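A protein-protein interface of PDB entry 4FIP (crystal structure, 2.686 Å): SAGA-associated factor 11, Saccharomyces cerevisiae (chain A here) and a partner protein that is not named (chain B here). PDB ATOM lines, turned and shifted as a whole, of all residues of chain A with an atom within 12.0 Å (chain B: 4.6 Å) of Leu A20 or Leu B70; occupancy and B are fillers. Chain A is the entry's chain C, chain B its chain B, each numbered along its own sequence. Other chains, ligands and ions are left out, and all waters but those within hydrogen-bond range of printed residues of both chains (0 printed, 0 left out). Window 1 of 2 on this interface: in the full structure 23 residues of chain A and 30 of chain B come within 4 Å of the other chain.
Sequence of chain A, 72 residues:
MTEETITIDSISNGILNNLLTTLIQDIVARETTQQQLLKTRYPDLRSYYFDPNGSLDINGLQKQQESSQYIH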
ATOM      1  N   ASP A   9      21.790 -21.126  -6.330  1.00  0.00           N
ATOM      2  CA  ASP A   9      22.300 -22.312  -7.042  1.00  0.00           C
ATOM      3  C   ASP A   9      21.192 -22.959  -7.862  1.00  0.00           C
ATOM      4  O   ASP A   9      21.410 -23.295  -9.020  1.00  0.00           O
ATOM      5  CB  ASP A   9      22.853 -23.384  -6.077  1.00  0.00           C
ATOM      6  CG  ASP A   9      24.092 -22.924  -5.283  1.00  0.00           C
ATOM      7  OD1 ASP A   9      25.137 -22.592  -5.891  1.00  0.00           O
ATOM      8  OD2 ASP A   9      24.027 -22.933  -4.029  1.00  0.00           O
ATOM      9  N   SER A  10      20.008 -23.121  -7.269  1.00  0.00           N
ATOM     10  CA  SER A  10      18.943 -23.887  -7.923  1.00  0.00           C
ATOM     11  C   SER A  10      18.355 -23.124  -9.084  1.00  0.00           C
ATOM     12  O   SER A  10      18.243 -23.657 -10.173  1.00  0.00           O
ATOM     13  CB  SER A  10      17.803 -24.291  -6.975  1.00  0.00           C
ATOM     14  OG  SER A  10      16.731 -23.349  -6.979  1.00  0.00           O
ATOM     15  N   ILE A  11      17.962 -21.879  -8.871  1.00  0.00           N
ATOM     16  CA  ILE A  11      17.328 -21.175  -9.948  1.00  0.00           C
ATOM     17  C   ILE A  11      18.370 -20.734 -10.972  1.00  0.00           C
ATOM     18  O   ILE A  11      18.016 -20.290 -12.060  1.00  0.00           O
ATOM     19  CB  ILE A  11      16.461 -20.000  -9.462  1.00  0.00           C
ATOM     20  CG1 ILE A  11      17.300 -18.736  -9.328  1.00  0.00           C
ATOM     21  CG2 ILE A  11      15.678 -20.379  -8.196  1.00  0.00           C
ATOM     22  CD1 ILE A  11      17.308 -17.924 -10.595  1.00  0.00           C
ATOM     23  N   SER A  12      19.656 -20.847 -10.635  1.00  0.00           N
ATOM     24  CA  SER A  12      20.703 -20.667 -11.632  1.00  0.00           C
ATOM     25  C   SER A  12      20.657 -21.834 -12.581  1.00  0.00           C
ATOM     26  O   SER A  12      20.802 -21.664 -13.784  1.00  0.00           O
ATOM     27  CB  SER A  12      22.082 -20.578 -11.001  1.00  0.00           C
ATOM     28  OG  SER A  12      22.251 -19.320 -10.383  1.00  0.00           O
ATOM     29  N   ASN A  13      20.432 -23.019 -12.032  1.00  0.00           N
ATOM     30  CA  ASN A  13      20.420 -24.240 -12.821  1.00  0.00           C
ATOM     31  C   ASN A  13      19.185 -24.381 -13.695  1.00  0.00           C
ATOM     32  O   ASN A  13      19.245 -24.973 -14.769  1.00  0.00           O
ATOM     33  CB  ASN A  13      20.595 -25.451 -11.914  1.00  0.00           C
ATOM     34  CG  ASN A  13      21.964 -25.476 -11.269  1.00  0.00           C
ATOM     35  OD1 ASN A  13      22.951 -25.115 -11.895  1.00  0.00           O
ATOM     36  ND2 ASN A  13      22.029 -25.880 -10.014  1.00  0.00           N
ATOM     37  N   GLY A  14      18.080 -23.812 -13.254  1.00  0.00           N
ATOM     38  CA  GLY A  14      16.884 -23.743 -14.078  1.00  0.00           C
ATOM     39  C   GLY A  14      17.157 -22.946 -15.337  1.00  0.00           C
ATOM     40  O   GLY A  14      16.769 -23.367 -16.427  1.00  0.00           O
ATOM     41  N   ILE A  15      17.845 -21.813 -15.184  1.00  0.00           N
ATOM     42  CA  ILE A  15      18.117 -20.920 -16.292  1.00  0.00           C
ATOM     43  C   ILE A  15      19.083 -21.526 -17.315  1.00  0.00           C
ATOM     44  O   ILE A  15      18.906 -21.336 -18.530  1.00  0.00           O
ATOM     45  CB  ILE A  15      18.724 -19.621 -15.788  1.00  0.00           C
ATOM     46  CG1 ILE A  15      17.632 -18.716 -15.234  1.00  0.00           C
ATOM     47  CG2 ILE A  15      19.447 -18.902 -16.913  1.00  0.00           C
ATOM     48  CD1 ILE A  15      18.182 -17.617 -14.340  1.00  0.00           C
ATOM     49  N   LEU A  16      20.106 -22.226 -16.808  1.00  0.00           N
ATOM     50  CA  LEU A  16      21.070 -22.956 -17.644  1.00  0.00           C
ATOM     51  C   LEU A  16      20.365 -24.110 -18.330  1.00  0.00           C
ATOM     52  O   LEU A  16      20.476 -24.300 -19.548  1.00  0.00           O
ATOM     53  CB  LEU A  16      22.239 -23.503 -16.810  1.00  0.00           C
ATOM     54  CG  LEU A  16      23.320 -24.261 -17.587  1.00  0.00           C
ATOM     55  CD1 LEU A  16      23.855 -23.449 -18.767  1.00  0.00           C
ATOM     56  CD2 LEU A  16      24.449 -24.644 -16.650  1.00  0.00           C
ATOM     57  N   ASN A  17      19.623 -24.879 -17.545  1.00  0.00           N
ATOM     58  CA  ASN A  17      18.817 -25.937 -18.105  1.00  0.00           C
ATOM     59  C   ASN A  17      17.909 -25.456 -19.229  1.00  0.00           C
ATOM     60  O   ASN A  17      17.702 -26.154 -20.201  1.00  0.00           O
ATOM     61  CB  ASN A  17      17.961 -26.544 -17.029  1.00  0.00           C
ATOM     62  CG  ASN A  17      17.299 -27.802 -17.480  1.00  0.00           C
ATOM     63  OD1 ASN A  17      17.965 -28.713 -17.913  1.00  0.00           O
ATOM     64  ND2 ASN A  17      15.980 -27.857 -17.384  1.00  0.00           N
ATOM     65  N   ASN A  18      17.350 -24.269 -19.091  1.00  0.00           N
ATOM     66  CA  ASN A  18      16.468 -23.773 -20.110  1.00  0.00           C
ATOM     67  C   ASN A  18      17.267 -23.498 -21.380  1.00  0.00           C
ATOM     68  O   ASN A  18      16.924 -23.964 -22.489  1.00  0.00           O
ATOM     69  CB  ASN A  18      15.709 -22.546 -19.604  1.00  0.00           C
ATOM     70  CG  ASN A  18      14.484 -22.928 -18.766  1.00  0.00           C
ATOM     71  OD1 ASN A  18      13.544 -22.143 -18.597  1.00  0.00           O
ATOM     72  ND2 ASN A  18      14.484 -24.149 -18.253  1.00  0.00           N
ATOM     73  N   LEU A  19      18.374 -22.792 -21.213  1.00  0.00           N
ATOM     74  CA  LEU A  19      19.218 -22.491 -22.354  1.00  0.00           C
ATOM     75  C   LEU A  19      19.684 -23.777 -23.081  1.00  0.00           C
ATOM     76  O   LEU A  19      19.559 -23.859 -24.303  1.00  0.00           O
ATOM     77  CB  LEU A  19      20.408 -21.619 -21.934  1.00  0.00           C
ATOM     78  CG  LEU A  19      20.085 -20.173 -21.565  1.00  0.00           C
ATOM     79  CD1 LEU A  19      21.211 -19.604 -20.708  1.00  0.00           C
ATOM     80  CD2 LEU A  19      19.832 -19.284 -22.765  1.00  0.00           C
ATOM     81  N   LEU A  20      20.203 -24.760 -22.331  1.00  0.00           N
ATOM     82  CA  LEU A  20      20.717 -26.016 -22.905  1.00  0.00           C
ATOM     83  C   LEU A  20      19.653 -26.776 -23.658  1.00  0.00           C
ATOM     84  O   LEU A  20      19.823 -27.055 -24.837  1.00  0.00           O
ATOM     85  CB  LEU A  20      21.303 -26.923 -21.804  1.00  0.00           C
ATOM     86  CG  LEU A  20      22.672 -26.435 -21.302  1.00  0.00           C
ATOM     87  CD1 LEU A  20      23.177 -27.221 -20.084  1.00  0.00           C
ATOM     88  CD2 LEU A  20      23.697 -26.427 -22.452  1.00  0.00           C
ATOM     89  N   THR A  21      18.547 -27.088 -22.974  1.00  0.00           N
ATOM     90  CA  THR A  21      17.448 -27.832 -23.565  1.00  0.00           C
ATOM     91  C   THR A  21      16.882 -27.133 -24.810  1.00  0.00           C
ATOM     92  O   THR A  21      16.575 -27.812 -25.797  1.00  0.00           O
ATOM     93  CB  THR A  21      16.333 -28.193 -22.534  1.00  0.00           C
ATOM     94  OG1 THR A  21      15.602 -27.039 -22.106  1.00  0.00           O
ATOM     95  CG2 THR A  21      16.964 -28.912 -21.330  1.00  0.00           C
ATOM     96  N   THR A  22      16.790 -25.799 -24.776  1.00  0.00           N
ATOM     97  CA  THR A  22      16.409 -25.023 -25.954  1.00  0.00           C
ATOM     98  C   THR A  22      17.394 -25.285 -27.097  1.00  0.00           C
ATOM     99  O   THR A  22      17.015 -25.684 -28.223  1.00  0.00           O
ATOM    100  CB  THR A  22      16.329 -23.501 -25.640  1.00  0.00           C
ATOM    101  OG1 THR A  22      15.383 -23.279 -24.578  1.00  0.00           O
ATOM    102  CG2 THR A  22      15.937 -22.678 -26.892  1.00  0.00           C
ATOM    103  N   LEU A  23      18.668 -25.108 -26.800  1.00  0.00           N
ATOM    104  CA  LEU A  23      19.697 -25.303 -27.804  1.00  0.00           C
ATOM    105  C   LEU A  23      19.683 -26.741 -28.351  1.00  0.00           C
ATOM    106  O   LEU A  23      19.662 -26.933 -29.567  1.00  0.00           O
ATOM    107  CB  LEU A  23      21.019 -24.994 -27.171  1.00  0.00           C
ATOM    108  CG  LEU A  23      22.206 -24.898 -28.094  1.00  0.00           C
ATOM    109  CD1 LEU A  23      21.785 -24.121 -29.331  1.00  0.00           C
ATOM    110  CD2 LEU A  23      23.359 -24.247 -27.320  1.00  0.00           C
ATOM    111  N   ILE A  24      19.656 -27.740 -27.458  1.00  0.00           N
ATOM    112  CA  ILE A  24      19.535 -29.145 -27.896  1.00  0.00           C
ATOM    113  C   ILE A  24      18.310 -29.366 -28.801  1.00  0.00           C
ATOM    114  O   ILE A  24      18.410 -29.985 -29.837  1.00  0.00           O
ATOM    115  CB  ILE A  24      19.394 -30.155 -26.725  1.00  0.00           C
ATOM    116  CG1 ILE A  24      20.645 -30.213 -25.854  1.00  0.00           C
ATOM    117  CG2 ILE A  24      19.127 -31.545 -27.254  1.00  0.00           C
ATOM    118  CD1 ILE A  24      20.384 -30.780 -24.454  1.00  0.00           C
ATOM    119  N   GLN A  25      17.154 -28.880 -28.370  1.00  0.00           N
ATOM    120  CA  GLN A  25      15.916 -29.090 -29.112  1.00  0.00           C
ATOM    121  C   GLN A  25      15.961 -28.397 -30.475  1.00  0.00           C
ATOM    122  O   GLN A  25      15.279 -28.845 -31.421  1.00  0.00           O
ATOM    123  CB  GLN A  25      14.736 -28.579 -28.327  1.00  0.00           C
ATOM    124  CG  GLN A  25      14.411 -29.458 -27.157  1.00  0.00           C
ATOM    125  CD  GLN A  25      13.485 -28.803 -26.163  1.00  0.00           C
ATOM    126  OE1 GLN A  25      13.647 -28.982 -24.944  1.00  0.00           O
ATOM    127  NE2 GLN A  25      12.488 -28.051 -26.674  1.00  0.00           N
ATOM    128  N   ASP A  26      16.762 -27.337 -30.591  1.00  0.00           N
ATOM    129  CA  ASP A  26      16.941 -26.710 -31.883  1.00  0.00           C
ATOM    130  C   ASP A  26      17.878 -27.528 -32.808  1.00  0.00           C
ATOM    131  O   ASP A  26      17.543 -27.767 -34.002  1.00  0.00           O
ATOM    132  CB  ASP A  26      17.427 -25.270 -31.743  1.00  0.00           C
ATOM    133  CG  ASP A  26      17.544 -24.567 -33.079  1.00  0.00           C
ATOM    134  OD1 ASP A  26      16.902 -25.005 -34.067  1.00  0.00           O
ATOM    135  OD2 ASP A  26      18.307 -23.577 -33.155  1.00  0.00           O
ATOM    136  N   ILE A  27      19.033 -27.947 -32.293  1.00  0.00           N
ATOM    137  CA  ILE A  27      19.922 -28.815 -33.074  1.00  0.00           C
ATOM    138  C   ILE A  27      19.134 -30.037 -33.582  1.00  0.00           C
ATOM    139  O   ILE A  27      19.055 -30.288 -34.806  1.00  0.00           O
ATOM    140  CB  ILE A  27      21.168 -29.258 -32.273  1.00  0.00           C
ATOM    141  CG1 ILE A  27      22.076 -28.068 -31.953  1.00  0.00           C
ATOM    142  CG2 ILE A  27      22.028 -30.237 -33.060  1.00  0.00           C
ATOM    143  CD1 ILE A  27      23.136 -28.343 -30.894  1.00  0.00           C
ATOM    144  N   VAL A  28      18.491 -30.758 -32.660  1.00  0.00           N
ATOM    145  CA  VAL A  28      17.727 -31.982 -33.026  1.00  0.00           C
ATOM    146  C   VAL A  28      16.645 -31.723 -34.109  1.00  0.00           C
ATOM    147  O   VAL A  28      16.485 -32.551 -35.011  1.00  0.00           O
ATOM    148  CB  VAL A  28      17.091 -32.692 -31.795  1.00  0.00           C
ATOM    149  CG1 VAL A  28      16.133 -33.777 -32.262  1.00  0.00           C
ATOM    150  CG2 VAL A  28      18.148 -33.277 -30.867  1.00  0.00           C
ATOM    151  N   ALA A  29      15.925 -30.591 -34.029  1.00  0.00           N
ATOM    152  CA  ALA A  29      14.837 -30.269 -34.998  1.00  0.00           C
ATOM    153  C   ALA A  29      15.392 -30.074 -36.406  1.00  0.00           C
ATOM    154  O   ALA A  29      14.810 -30.550 -37.375  1.00  0.00           O
ATOM    155  CB  ALA A  29      14.040 -29.039 -34.562  1.00  0.00           C
ATOM    156  N   ARG A  30      16.537 -29.406 -36.507  1.00  0.00           N
ATOM    157  CA  ARG A  30      17.196 -29.215 -37.782  1.00  0.00           C
ATOM    158  C   ARG A  30      17.729 -30.511 -38.340  1.00  0.00           C
ATOM    159  O   ARG A  30      17.681 -30.716 -39.521  1.00  0.00           O
ATOM    160  CB  ARG A  30      18.353 -28.268 -37.625  1.00  0.00           C
ATOM    161  CG  ARG A  30      17.967 -26.861 -37.176  1.00  0.00           C
ATOM    162  CD  ARG A  30      19.183 -26.033 -36.803  1.00  0.00           C
ATOM    163  NE  ARG A  30      18.811 -24.742 -36.212  1.00  0.00           N
ATOM    164  CZ  ARG A  30      18.747 -23.601 -36.893  1.00  0.00           C
ATOM    165  NH1 ARG A  30      19.010 -23.565 -38.186  1.00  0.00           N
ATOM    166  NH2 ARG A  30      18.420 -22.484 -36.281  1.00  0.00           N
ATOM    167  N   LEU B  29      27.467 -18.872 -23.817  1.00  0.00           N
ATOM    168  CA  LEU B  29      27.222 -20.313 -23.776  1.00  0.00           C
ATOM    169  C   LEU B  29      27.314 -20.951 -25.181  1.00  0.00           C
ATOM    170  O   LEU B  29      28.097 -21.884 -25.385  1.00  0.00           O
ATOM    171  CB  LEU B  29      25.886 -20.612 -23.115  1.00  0.00           C
ATOM    172  CG  LEU B  29      25.478 -22.084 -22.999  1.00  0.00           C
ATOM    173  CD1 LEU B  29      26.346 -22.776 -21.960  1.00  0.00           C
ATOM    174  CD2 LEU B  29      23.985 -22.232 -22.681  1.00  0.00           C
ATOM    175  N   LEU B  33      30.226 -23.726 -26.306  1.00  0.00           N
ATOM    176  CA  LEU B  33      29.772 -25.059 -26.652  1.00  0.00           C
ATOM    177  C   LEU B  33      30.265 -25.431 -28.031  1.00  0.00           C
ATOM    178  O   LEU B  33      30.638 -26.586 -28.286  1.00  0.00           O
ATOM    179  CB  LEU B  33      28.261 -25.140 -26.592  1.00  0.00           C
ATOM    180  CG  LEU B  33      27.640 -25.082 -25.192  1.00  0.00           C
ATOM    181  CD1 LEU B  33      26.114 -25.100 -25.330  1.00  0.00           C
ATOM    182  CD2 LEU B  33      28.151 -26.189 -24.275  1.00  0.00           C
ATOM    183  N   GLU B  66      18.400 -36.056 -25.662  1.00  0.00           N
ATOM    184  CA  GLU B  66      18.446 -34.884 -24.774  1.00  0.00           C
ATOM    185  C   GLU B  66      19.186 -35.139 -23.472  1.00  0.00           C
ATOM    186  O   GLU B  66      19.999 -34.314 -23.050  1.00  0.00           O
ATOM    187  CB  GLU B  66      17.056 -34.332 -24.487  1.00  0.00           C
ATOM    188  CG  GLU B  66      17.126 -33.003 -23.780  1.00  0.00           C
ATOM    189  CD  GLU B  66      15.779 -32.351 -23.628  1.00  0.00           C
ATOM    190  OE1 GLU B  66      14.978 -32.767 -22.757  1.00  0.00           O
ATOM    191  OE2 GLU B  66      15.521 -31.397 -24.374  1.00  0.00           O
ATOM    192  N   PRO B  67      18.925 -36.283 -22.840  1.00  0.00           N
ATOM    193  CA  PRO B  67      19.653 -36.563 -21.607  1.00  0.00           C
ATOM    194  C   PRO B  67      21.162 -36.758 -21.829  1.00  0.00           C
ATOM    195  O   PRO B  67      21.953 -36.313 -21.000  1.00  0.00           O
ATOM    196  CB  PRO B  67      19.004 -37.837 -21.099  1.00  0.00           C
ATOM    197  CG  PRO B  67      17.742 -38.005 -21.900  1.00  0.00           C
ATOM    198  CD  PRO B  67      18.039 -37.389 -23.220  1.00  0.00           C
ATOM    199  N   LYS B  68      21.551 -37.394 -22.937  1.00  0.00           N
ATOM    200  CA  LYS B  68      22.958 -37.592 -23.261  1.00  0.00           C
ATOM    201  C   LYS B  68      23.658 -36.293 -23.669  1.00  0.00           C
ATOM    202  O   LYS B  68      24.863 -36.153 -23.470  1.00  0.00           O
ATOM    203  CB  LYS B  68      23.125 -38.660 -24.340  1.00  0.00           C
ATOM    204  CG  LYS B  68      23.362 -40.066 -23.778  1.00  0.00           C
ATOM    205  CD  LYS B  68      23.607 -41.142 -24.839  1.00  0.00           C
ATOM    206  CE  LYS B  68      22.344 -41.936 -25.152  1.00  0.00           C
ATOM    207  NZ  LYS B  68      22.546 -42.991 -26.195  1.00  0.00           N
ATOM    208  N   ALA B  69      22.920 -35.349 -24.248  1.00  0.00           N
ATOM    209  CA  ALA B  69      23.502 -34.067 -24.604  1.00  0.00           C
ATOM    210  C   ALA B  69      23.706 -33.236 -23.348  1.00  0.00           C
ATOM    211  O   ALA B  69      24.656 -32.487 -23.245  1.00  0.00           O
ATOM    212  CB  ALA B  69      22.640 -33.328 -25.601  1.00  0.00           C
ATOM    213  N   LEU B  70      22.832 -33.356 -22.366  1.00  0.00           N
ATOM    214  CA  LEU B  70      23.062 -32.620 -21.104  1.00  0.00           C
ATOM    215  C   LEU B  70      24.236 -33.248 -20.312  1.00  0.00           C
ATOM    216  O   LEU B  70      25.039 -32.548 -19.704  1.00  0.00           O
ATOM    217  CB  LEU B  70      21.785 -32.558 -20.256  1.00  0.00           C
ATOM    218  CG  LEU B  70      20.469 -32.040 -20.869  1.00  0.00           C
ATOM    219  CD1 LEU B  70      19.273 -32.333 -19.969  1.00  0.00           C
ATOM    220  CD2 LEU B  70      20.536 -30.555 -21.184  1.00  0.00           C
ATOM    221  N   GLU B  71      24.350 -34.567 -20.354  1.00  0.00           N
ATOM    222  CA  GLU B  71      25.473 -35.254 -19.721  1.00  0.00           C
ATOM    223  C   GLU B  71      26.788 -34.839 -20.386  1.00  0.00           C
ATOM    224  O   GLU B  71      27.852 -34.883 -19.758  1.00  0.00           O
ATOM    225  CB  GLU B  71      25.279 -36.783 -19.777  1.00  0.00           C
ATOM    226  CG  GLU B  71      24.169 -37.283 -18.843  1.00  0.00           C
ATOM    227  CD  GLU B  71      23.555 -38.641 -19.225  1.00  0.00           C
ATOM    228  OE1 GLU B  71      23.774 -39.129 -20.362  1.00  0.00           O
ATOM    229  OE2 GLU B  71      22.823 -39.228 -18.374  1.00  0.00           O
ATOM    230  N   MET B  72      26.699 -34.409 -21.642  1.00  0.00           N
ATOM    231  CA  MET B  72      27.882 -34.123 -22.459  1.00  0.00           C
ATOM    232  C   MET B  72      28.545 -32.745 -22.269  1.00  0.00           C
ATOM    233  O   MET B  72      29.649 -32.563 -22.732  1.00  0.00           O
ATOM    234  CB  MET B  72      27.546 -34.301 -23.948  1.00  0.00           C
ATOM    235  CG  MET B  72      27.805 -35.691 -24.494  1.00  0.00           C
ATOM    236  SD  MET B  72      27.191 -35.945 -26.180  1.00  0.00           S
ATOM    237  CE  MET B  72      27.825 -34.505 -27.030  1.00  0.00           C
ATOM    238  N   VAL B  73      27.906 -31.765 -21.636  1.00  0.00           N
ATOM    239  CA  VAL B  73      28.556 -30.433 -21.510  1.00  0.00           C
ATOM    240  C   VAL B  73      29.714 -30.572 -20.524  1.00  0.00           C
ATOM    241  O   VAL B  73      29.600 -31.306 -19.563  1.00  0.00           O
ATOM    242  CB  VAL B  73      27.601 -29.281 -21.083  1.00  0.00           C
ATOM    243  CG1 VAL B  73      26.207 -29.461 -21.656  1.00  0.00           C
ATOM    244  CG2 VAL B  73      27.506 -29.192 -19.587  1.00  0.00           C
ATOM    245  N   ARG B  78      29.986 -25.616 -17.787  1.00  0.00           N
ATOM    246  CA  ARG B  78      28.986 -25.692 -16.703  1.00  0.00           C
ATOM    247  C   ARG B  78      29.356 -24.847 -15.479  1.00  0.00           C
ATOM    248  O   ARG B  78      28.544 -24.042 -15.049  1.00  0.00           O
ATOM    249  CB  ARG B  78      28.717 -27.176 -16.334  1.00  0.00           C
ATOM    250  CG  ARG B  78      28.154 -27.496 -14.944  1.00  0.00           C
ATOM    251  CD  ARG B  78      27.476 -28.868 -14.921  1.00  0.00           C
ATOM    252  NE  ARG B  78      26.176 -28.837 -15.625  1.00  0.00           N
ATOM    253  CZ  ARG B  78      25.768 -29.662 -16.603  1.00  0.00           C
ATOM    254  NH1 ARG B  78      26.522 -30.660 -17.053  1.00  0.00           N
ATOM    255  NH2 ARG B  78      24.559 -29.494 -17.136  1.00  0.00           N
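OE1 of Gln A25 lies close to OE2 of Glu B66.
OE1 of Gln A25 lies close to O of Thr A21, at 3.3 Å. O of Asn A17 lies within hydrogen-bond range of OG1 of Thr A21 (3.0 Å). The backbone carbonyl oxygen of Asn A18 sits at hydrogen-bond distance from the side-chain hydroxyl of Thr A21 (3.4 Å).
Leu A19 touches Leu B29. Leu B33 touches Leu A20. Leu A20 touches Leu B70. Leu A20 touches Arg B78. Glu B66 touches Thr A21 (OE2 to CB, 3.8 Å). Leu B70 touches Thr A21. CD2 of Leu A23 touches CD1 of Leu B33 (3.5 Å). Ile A24 touches Glu B66 (CD1 to O, 3.8 Å). Ala B69 touches Ile A24 (CB to CD1, 3.6 Å). Ile A24 touches Leu B70 (CD1 to CD2, 3.3 Å).
Asn A18 touches none of the printed residues of chain B. Of the printed residues of chain B, Leu A20 touches Leu B33, Leu B70 and Arg B78. Of the printed residues of chain B, Gln A25 touches Glu B66. Ile A27 touches none of the printed residues of chain B. Printed residues of chain A within 4 Å of Leu B29: Leu A19. Glu B66 touches just these residues of chain A: Thr A21 (3.8 Å), Ile A24 (3.8 Å) and Gln A25 (3.1 Å). No residue of chain A comes within 4 Å of Pro B67. Of chain A, only Ile A24 comes within 4 Å of Ala B69. No residue of chain A comes within 4 Å of Glu B71. No residue of chain A comes within 4 Å of Met B72. Printed residues of chain A within 4 Å of Arg B78: Leu A20. The nearest residue of chain A that does not touch Leu B70 is Asn A17 (4.4 Å).
Hydrophobic or aromatic side chains of chain B that line the printed part of chain A: Leu B29, Leu B33, Ala B69 and Leu B70. Of the 22 printed residues of chain A, 6 touch a printed residue of chain B. Hydrophobic or aromatic side chains of chain A within 4 Å of the printed part of chain B: Leu A19, Leu A20, Leu A23 and Ile A24. Among the printed residues, 11 pairs touch across the chains. Among the printed residues, no Asp or Glu carboxylate lies within 4 Å of a Lys or Arg side-chain nitrogen of the other chain.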
